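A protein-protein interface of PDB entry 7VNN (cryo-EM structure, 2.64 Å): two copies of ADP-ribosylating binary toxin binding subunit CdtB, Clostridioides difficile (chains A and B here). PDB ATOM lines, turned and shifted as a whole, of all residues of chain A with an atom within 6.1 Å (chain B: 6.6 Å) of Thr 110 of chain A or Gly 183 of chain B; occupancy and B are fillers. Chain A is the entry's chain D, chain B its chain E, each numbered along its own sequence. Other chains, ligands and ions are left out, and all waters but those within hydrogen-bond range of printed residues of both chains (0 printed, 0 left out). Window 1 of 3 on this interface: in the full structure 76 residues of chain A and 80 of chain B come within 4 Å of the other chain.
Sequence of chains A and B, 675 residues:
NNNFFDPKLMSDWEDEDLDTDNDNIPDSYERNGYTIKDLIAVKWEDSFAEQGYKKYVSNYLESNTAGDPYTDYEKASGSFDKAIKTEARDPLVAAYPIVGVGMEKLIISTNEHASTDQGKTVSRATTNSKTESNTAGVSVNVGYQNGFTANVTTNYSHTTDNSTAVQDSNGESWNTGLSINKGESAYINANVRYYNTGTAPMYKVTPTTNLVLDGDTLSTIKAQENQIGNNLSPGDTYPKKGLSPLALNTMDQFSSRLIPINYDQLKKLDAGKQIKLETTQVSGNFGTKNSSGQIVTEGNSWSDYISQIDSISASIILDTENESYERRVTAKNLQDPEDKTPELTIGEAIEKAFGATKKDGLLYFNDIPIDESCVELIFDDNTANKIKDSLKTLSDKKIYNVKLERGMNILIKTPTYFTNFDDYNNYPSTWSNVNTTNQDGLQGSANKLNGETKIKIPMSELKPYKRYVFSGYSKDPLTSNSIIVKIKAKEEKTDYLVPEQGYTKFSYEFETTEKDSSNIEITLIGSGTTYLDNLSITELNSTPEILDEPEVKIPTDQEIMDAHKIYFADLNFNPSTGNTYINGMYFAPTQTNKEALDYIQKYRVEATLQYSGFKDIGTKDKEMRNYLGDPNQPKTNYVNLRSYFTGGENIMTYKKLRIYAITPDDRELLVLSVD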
ATOM      1  N   ILE A 108     -13.606  14.991 -17.288  1.00  0.00           N
ATOM      2  CA  ILE A 108     -13.328  14.455 -15.960  1.00  0.00           C
ATOM      3  C   ILE A 108     -11.989  13.733 -16.000  1.00  0.00           C
ATOM      4  O   ILE A 108     -11.751  12.905 -16.886  1.00  0.00           O
ATOM      5  CB  ILE A 108     -14.445  13.506 -15.489  1.00  0.00           C
ATOM      6  CG1 ILE A 108     -15.815  14.128 -15.757  1.00  0.00           C
ATOM      7  CG2 ILE A 108     -14.283  13.183 -14.017  1.00  0.00           C
ATOM      8  CD1 ILE A 108     -16.950  13.134 -15.743  1.00  0.00           C
ATOM      9  N   SER A 109     -11.121  14.048 -15.043  1.00  0.00           N
ATOM     10  CA  SER A 109      -9.798  13.435 -14.924  1.00  0.00           C
ATOM     11  C   SER A 109      -9.743  12.683 -13.600  1.00  0.00           C
ATOM     12  O   SER A 109      -9.480  13.280 -12.552  1.00  0.00           O
ATOM     13  CB  SER A 109      -8.696  14.488 -15.007  1.00  0.00           C
ATOM     14  OG  SER A 109      -8.684  15.118 -16.274  1.00  0.00           O
ATOM     15  N   THR A 110      -9.981  11.375 -13.648  1.00  0.00           N
ATOM     16  CA  THR A 110     -10.020  10.576 -12.431  1.00  0.00           C
ATOM     17  C   THR A 110      -8.627  10.481 -11.820  1.00  0.00           C
ATOM     18  O   THR A 110      -7.653  10.172 -12.512  1.00  0.00           O
ATOM     19  CB  THR A 110     -10.569   9.184 -12.726  1.00  0.00           C
ATOM     20  OG1 THR A 110     -11.851   9.301 -13.355  1.00  0.00           O
ATOM     21  CG2 THR A 110     -10.736   8.405 -11.438  1.00  0.00           C
ATOM     22  N   ASN A 111      -8.537  10.740 -10.517  1.00  0.00           N
ATOM     23  CA  ASN A 111      -7.257  10.866  -9.821  1.00  0.00           C
ATOM     24  C   ASN A 111      -6.950   9.555  -9.099  1.00  0.00           C
ATOM     25  O   ASN A 111      -7.252   9.372  -7.920  1.00  0.00           O
ATOM     26  CB  ASN A 111      -7.299  12.054  -8.864  1.00  0.00           C
ATOM     27  CG  ASN A 111      -6.031  12.199  -8.055  1.00  0.00           C
ATOM     28  OD1 ASN A 111      -4.934  11.935  -8.544  1.00  0.00           O
ATOM     29  ND2 ASN A 111      -6.176  12.632  -6.808  1.00  0.00           N
ATOM     30  N   GLU A 112      -6.330   8.633  -9.829  1.00  0.00           N
ATOM     31  CA  GLU A 112      -5.970   7.327  -9.303  1.00  0.00           C
ATOM     32  C   GLU A 112      -4.468   7.109  -9.416  1.00  0.00           C
ATOM     33  O   GLU A 112      -3.786   7.733 -10.232  1.00  0.00           O
ATOM     34  CB  GLU A 112      -6.705   6.203 -10.043  1.00  0.00           C
ATOM     35  CG  GLU A 112      -8.209   6.246  -9.909  1.00  0.00           C
ATOM     36  CD  GLU A 112      -8.910   5.516 -11.037  1.00  0.00           C
ATOM     37  OE1 GLU A 112      -8.416   5.578 -12.184  1.00  0.00           O
ATOM     38  OE2 GLU A 112      -9.953   4.881 -10.779  1.00  0.00           O
ATOM     39  N   ILE A 180      -6.761   5.265  -4.330  1.00  0.00           N
ATOM     40  CA  ILE A 180      -7.754   6.301  -4.579  1.00  0.00           C
ATOM     41  C   ILE A 180      -7.870   7.178  -3.342  1.00  0.00           C
ATOM     42  O   ILE A 180      -7.587   6.746  -2.219  1.00  0.00           O
ATOM     43  CB  ILE A 180      -9.125   5.697  -4.961  1.00  0.00           C
ATOM     44  CG1 ILE A 180     -10.072   6.774  -5.497  1.00  0.00           C
ATOM     45  CG2 ILE A 180      -9.753   4.999  -3.768  1.00  0.00           C
ATOM     46  CD1 ILE A 180      -9.589   7.455  -6.753  1.00  0.00           C
ATOM     47  N   SER A 185     -11.364  12.722  -5.715  1.00  0.00           N
ATOM     48  CA  SER A 185     -11.326  11.562  -6.593  1.00  0.00           C
ATOM     49  C   SER A 185     -11.069  11.918  -8.048  1.00  0.00           C
ATOM     50  O   SER A 185     -10.525  11.088  -8.784  1.00  0.00           O
ATOM     51  CB  SER A 185     -12.637  10.780  -6.487  1.00  0.00           C
ATOM     52  OG  SER A 185     -12.827  10.290  -5.172  1.00  0.00           O
ATOM     53  N   ALA A 186     -11.437  13.121  -8.479  1.00  0.00           N
ATOM     54  CA  ALA A 186     -11.256  13.506  -9.870  1.00  0.00           C
ATOM     55  C   ALA A 186     -11.196  15.022  -9.962  1.00  0.00           C
ATOM     56  O   ALA A 186     -11.590  15.736  -9.039  1.00  0.00           O
ATOM     57  CB  ALA A 186     -12.378  12.958 -10.757  1.00  0.00           C
ATOM     58  N   TYR A 187     -10.688  15.500 -11.096  1.00  0.00           N
ATOM     59  CA  TYR A 187     -10.620  16.920 -11.405  1.00  0.00           C
ATOM     60  C   TYR A 187     -11.439  17.186 -12.657  1.00  0.00           C
ATOM     61  O   TYR A 187     -11.308  16.466 -13.651  1.00  0.00           O
ATOM     62  CB  TYR A 187      -9.173  17.377 -11.608  1.00  0.00           C
ATOM     63  CG  TYR A 187      -8.303  17.221 -10.383  1.00  0.00           C
ATOM     64  CD1 TYR A 187      -8.570  17.933  -9.225  1.00  0.00           C
ATOM     65  CD2 TYR A 187      -7.215  16.361 -10.386  1.00  0.00           C
ATOM     66  CE1 TYR A 187      -7.779  17.795  -8.103  1.00  0.00           C
ATOM     67  CE2 TYR A 187      -6.417  16.215  -9.269  1.00  0.00           C
ATOM     68  CZ  TYR A 187      -6.704  16.934  -8.130  1.00  0.00           C
ATOM     69  OH  TYR A 187      -5.913  16.793  -7.015  1.00  0.00           O
ATOM     70  N   LEU A 266     -18.374  11.817  -8.000  1.00  0.00           N
ATOM     71  CA  LEU A 266     -17.841  11.096  -9.150  1.00  0.00           C
ATOM     72  C   LEU A 266     -18.722   9.908  -9.515  1.00  0.00           C
ATOM     73  O   LEU A 266     -18.932   9.622 -10.698  1.00  0.00           O
ATOM     74  CB  LEU A 266     -16.409  10.642  -8.868  1.00  0.00           C
ATOM     75  CG  LEU A 266     -15.709   9.889  -9.997  1.00  0.00           C
ATOM     76  CD1 LEU A 266     -15.579  10.769 -11.222  1.00  0.00           C
ATOM     77  CD2 LEU A 266     -14.348   9.413  -9.542  1.00  0.00           C
ATOM     78  N   ASP A 270     -20.619   9.294 -13.042  1.00  0.00           N
ATOM     79  CA  ASP A 270     -20.452   8.075 -13.822  1.00  0.00           C
ATOM     80  C   ASP A 270     -21.766   7.342 -14.051  1.00  0.00           C
ATOM     81  O   ASP A 270     -21.813   6.427 -14.878  1.00  0.00           O
ATOM     82  CB  ASP A 270     -19.446   7.149 -13.138  1.00  0.00           C
ATOM     83  CG  ASP A 270     -18.011   7.517 -13.455  1.00  0.00           C
ATOM     84  OD1 ASP A 270     -17.801   8.366 -14.346  1.00  0.00           O
ATOM     85  OD2 ASP A 270     -17.095   6.965 -12.812  1.00  0.00           O
ATOM     86  N   ASN B 181       0.272   8.211 -12.297  1.00  0.00           N
ATOM     87  CA  ASN B 181      -0.861   8.983 -11.801  1.00  0.00           C
ATOM     88  C   ASN B 181      -1.784   9.242 -12.983  1.00  0.00           C
ATOM     89  O   ASN B 181      -1.357   9.804 -13.996  1.00  0.00           O
ATOM     90  CB  ASN B 181      -0.402  10.291 -11.161  1.00  0.00           C
ATOM     91  CG  ASN B 181      -1.479  10.935 -10.312  1.00  0.00           C
ATOM     92  OD1 ASN B 181      -2.647  10.554 -10.374  1.00  0.00           O
ATOM     93  ND2 ASN B 181      -1.092  11.926  -9.519  1.00  0.00           N
ATOM     94  N   LYS B 182      -3.046   8.828 -12.859  1.00  0.00           N
ATOM     95  CA  LYS B 182      -3.977   8.973 -13.970  1.00  0.00           C
ATOM     96  C   LYS B 182      -4.444  10.409 -14.154  1.00  0.00           C
ATOM     97  O   LYS B 182      -4.787  10.795 -15.276  1.00  0.00           O
ATOM     98  CB  LYS B 182      -5.177   8.053 -13.767  1.00  0.00           C
ATOM     99  CG  LYS B 182      -4.797   6.601 -13.555  1.00  0.00           C
ATOM    100  CD  LYS B 182      -4.196   6.001 -14.810  1.00  0.00           C
ATOM    101  CE  LYS B 182      -4.515   4.525 -14.912  1.00  0.00           C
ATOM    102  NZ  LYS B 182      -5.975   4.276 -14.782  1.00  0.00           N
ATOM    103  N   GLY B 183      -4.475  11.201 -13.088  1.00  0.00           N
ATOM    104  CA  GLY B 183      -4.850  12.596 -13.195  1.00  0.00           C
ATOM    105  C   GLY B 183      -3.852  13.421 -13.979  1.00  0.00           C
ATOM    106  O   GLY B 183      -4.237  14.241 -14.816  1.00  0.00           O
ATOM    107  N   GLU B 184      -2.563  13.216 -13.710  1.00  0.00           N
ATOM    108  CA  GLU B 184      -1.478  13.909 -14.404  1.00  0.00           C
ATOM    109  C   GLU B 184      -0.488  12.848 -14.873  1.00  0.00           C
ATOM    110  O   GLU B 184       0.488  12.548 -14.179  1.00  0.00           O
ATOM    111  CB  GLU B 184      -0.808  14.940 -13.501  1.00  0.00           C
ATOM    112  CG  GLU B 184      -1.772  15.855 -12.769  1.00  0.00           C
ATOM    113  CD  GLU B 184      -1.083  17.063 -12.172  1.00  0.00           C
ATOM    114  OE1 GLU B 184       0.164  17.071 -12.119  1.00  0.00           O
ATOM    115  OE2 GLU B 184      -1.788  18.007 -11.759  1.00  0.00           O
ATOM    116  N   SER B 185      -0.735  12.286 -16.053  1.00  0.00           N
ATOM    117  CA  SER B 185       0.119  11.236 -16.588  1.00  0.00           C
ATOM    118  C   SER B 185       1.308  11.771 -17.370  1.00  0.00           C
ATOM    119  O   SER B 185       2.282  11.035 -17.563  1.00  0.00           O
ATOM    120  CB  SER B 185      -0.694  10.299 -17.484  1.00  0.00           C
ATOM    121  OG  SER B 185      -1.826   9.796 -16.798  1.00  0.00           O
ATOM    122  N   ALA B 186       1.258  13.021 -17.823  1.00  0.00           N
ATOM    123  CA  ALA B 186       2.361  13.585 -18.586  1.00  0.00           C
ATOM    124  C   ALA B 186       2.273  15.103 -18.560  1.00  0.00           C
ATOM    125  O   ALA B 186       1.222  15.679 -18.269  1.00  0.00           O
ATOM    126  CB  ALA B 186       2.365  13.075 -20.030  1.00  0.00           C
ATOM    127  N   PRO B 260      -0.377  19.754 -17.161  1.00  0.00           N
ATOM    128  CA  PRO B 260      -0.621  18.312 -17.150  1.00  0.00           C
ATOM    129  C   PRO B 260      -1.692  17.896 -18.148  1.00  0.00           C
ATOM    130  O   PRO B 260      -2.504  18.698 -18.612  1.00  0.00           O
ATOM    131  CB  PRO B 260      -1.093  18.065 -15.712  1.00  0.00           C
ATOM    132  CG  PRO B 260      -1.803  19.337 -15.342  1.00  0.00           C
ATOM    133  CD  PRO B 260      -1.241  20.460 -16.199  1.00  0.00           C
ATOM    134  N   ILE B 261      -1.679  16.603 -18.471  1.00  0.00           N
ATOM    135  CA  ILE B 261      -2.691  16.001 -19.326  1.00  0.00           C
ATOM    136  C   ILE B 261      -3.203  14.734 -18.660  1.00  0.00           C
ATOM    137  O   ILE B 261      -2.575  14.174 -17.759  1.00  0.00           O
ATOM    138  CB  ILE B 261      -2.168  15.687 -20.745  1.00  0.00           C
ATOM    139  CG1 ILE B 261      -0.961  14.752 -20.681  1.00  0.00           C
ATOM    140  CG2 ILE B 261      -1.825  16.966 -21.489  1.00  0.00           C
ATOM    141  CD1 ILE B 261      -0.568  14.183 -22.024  1.00  0.00           C
ATOM    142  N   ASN B 262      -4.361  14.283 -19.125  1.00  0.00           N
ATOM    143  CA  ASN B 262      -5.027  13.110 -18.577  1.00  0.00           C
ATOM    144  C   ASN B 262      -4.293  11.845 -19.020  1.00  0.00           C
ATOM    145  O   ASN B 262      -3.258  11.888 -19.690  1.00  0.00           O
ATOM    146  CB  ASN B 262      -6.485  13.092 -19.021  1.00  0.00           C
ATOM    147  CG  ASN B 262      -7.410  12.542 -17.968  1.00  0.00           C
ATOM    148  OD1 ASN B 262      -7.013  11.730 -17.134  1.00  0.00           O
ATOM    149  ND2 ASN B 262      -8.662  12.977 -18.003  1.00  0.00           N
ATOM    150  N   TYR B 263      -4.837  10.690 -18.641  1.00  0.00           N
ATOM    151  CA  TYR B 263      -4.343   9.407 -19.125  1.00  0.00           C
ATOM    152  C   TYR B 263      -4.920   9.055 -20.490  1.00  0.00           C
ATOM    153  O   TYR B 263      -4.190   8.588 -21.371  1.00  0.00           O
ATOM    154  CB  TYR B 263      -4.675   8.304 -18.118  1.00  0.00           C
ATOM    155  CG  TYR B 263      -4.098   6.955 -18.470  1.00  0.00           C
ATOM    156  CD1 TYR B 263      -2.725   6.760 -18.539  1.00  0.00           C
ATOM    157  CD2 TYR B 263      -4.926   5.876 -18.741  1.00  0.00           C
ATOM    158  CE1 TYR B 263      -2.195   5.530 -18.863  1.00  0.00           C
ATOM    159  CE2 TYR B 263      -4.406   4.641 -19.066  1.00  0.00           C
ATOM    160  CZ  TYR B 263      -3.040   4.474 -19.126  1.00  0.00           C
ATOM    161  OH  TYR B 263      -2.520   3.243 -19.450  1.00  0.00           O
ATOM    162  N   GLN B 265      -6.006  11.257 -22.624  1.00  0.00           N
ATOM    163  CA  GLN B 265      -5.387  12.209 -23.539  1.00  0.00           C
ATOM    164  C   GLN B 265      -3.981  11.768 -23.927  1.00  0.00           C
ATOM    165  O   GLN B 265      -3.573  11.916 -25.084  1.00  0.00           O
ATOM    166  CB  GLN B 265      -5.365  13.600 -22.908  1.00  0.00           C
ATOM    167  CG  GLN B 265      -6.740  14.239 -22.791  1.00  0.00           C
ATOM    168  CD  GLN B 265      -6.804  15.302 -21.714  1.00  0.00           C
ATOM    169  OE1 GLN B 265      -5.820  15.563 -21.025  1.00  0.00           O
ATOM    170  NE2 GLN B 265      -7.967  15.921 -21.563  1.00  0.00           N
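The side-chain amide oxygen of Asn 181 of chain B lies close to the backbone carbonyl oxygen of Glu 112 of chain A (3.0 Å). The backbone carbonyl oxygen (O) of Thr 110 of chain A sits at hydrogen-bond distance from the backbone NH (N) of Gly 183 of chain B (3.4 Å). The side-chain amino group (NZ) of Lys 182 of chain B is in salt-bridge range of the side-chain carboxylate (OE1) of Glu 112 of chain A, 3.8 Å away. OD1 of Asn 181 of chain B lies close to OD1 of Asn 111 of chain A, 3.2 Å away. The backbone carbonyl oxygen (O) of Ile 108 of chain A is in hydrogen-bond range of the side-chain amide nitrogen (ND2) of Asn 262 of chain B, at 3.3 Å. ND2 of Asn 262 of chain B lies within hydrogen-bond range of OG of Ser 109 of chain A (2.8 Å).
The side-chain amide oxygen (OE1) of Gln 265 of chain B lies within hydrogen-bond range of the backbone NH (N) of Asn 262 of chain B (2.7 Å). The side-chain hydroxyl of Ser 185 of chain B lies within hydrogen-bond range of the backbone carbonyl oxygen of Asn 181 of chain B, at 2.8 Å. The side-chain amide oxygen of Asn 262 of chain B sits close to the backbone carbonyl oxygen of Lys 182 of chain B, 3.0 Å away. The backbone NH of Gly 183 of chain B lies close to the side-chain amide oxygen of Asn 181 of chain B (3.3 Å). N of Asn 111 of chain A lies within hydrogen-bond range of O of Ser 185 of chain A (2.7 Å). The backbone NH of Ser 109 of chain A sits at hydrogen-bond distance from the backbone carbonyl oxygen of Tyr 187 of chain A (2.8 Å).
O of Thr 110 of chain A touches CB of Lys 182 of chain B, 3.5 Å away.
Printed residues of chain B within 4 Å of Ile 108 of chain A: Asn 262 (3.3 Å). Of the printed residues of chain B, Thr 110 of chain A touches Lys 182 (3.5 Å) and Gly 183 (3.4 Å). Printed residues of chain B within 4 Å of Asn 111 of chain A: Asn 181. Asp 270 of chain A touches none of the printed residues of chain B. Printed residues of chain A within 4 Å of Asn 181 of chain B: Asn 111 (3.2 Å) and Glu 112 (3.0 Å). Of chain A, only Thr 110 (3.4 Å) comes within 4 Å of Gly 183 of chain B. Printed residues of chain A within 4 Å of Asn 262 of chain B: Ile 108 and Ser 109. The nearest residue of chain A that does not touch Gly 183 of chain B is Asn 111 of chain A (4.3 Å).
Printed residues of chain B that touch a printed residue of chain A: Asn 181, Lys 182, Gly 183 and Asn 262. Along chain B the printed residues that touch a printed residue of chain A span positions 181 to 262. Of the 11 printed residues of chain A, 5 touch a printed residue of chain B. Printed residues of chain A that touch a printed residue of chain B: Ile 108, Ser 109, Thr 110, Asn 111 and Glu 112. Along chain A the printed residues that touch a printed residue of chain B span positions 108 to 112.
Positions printed for both chains: 185 and 186. Of the 7 pairs that touch across the chains among the printed residues, none has its exchanged pair printed and touching as well.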
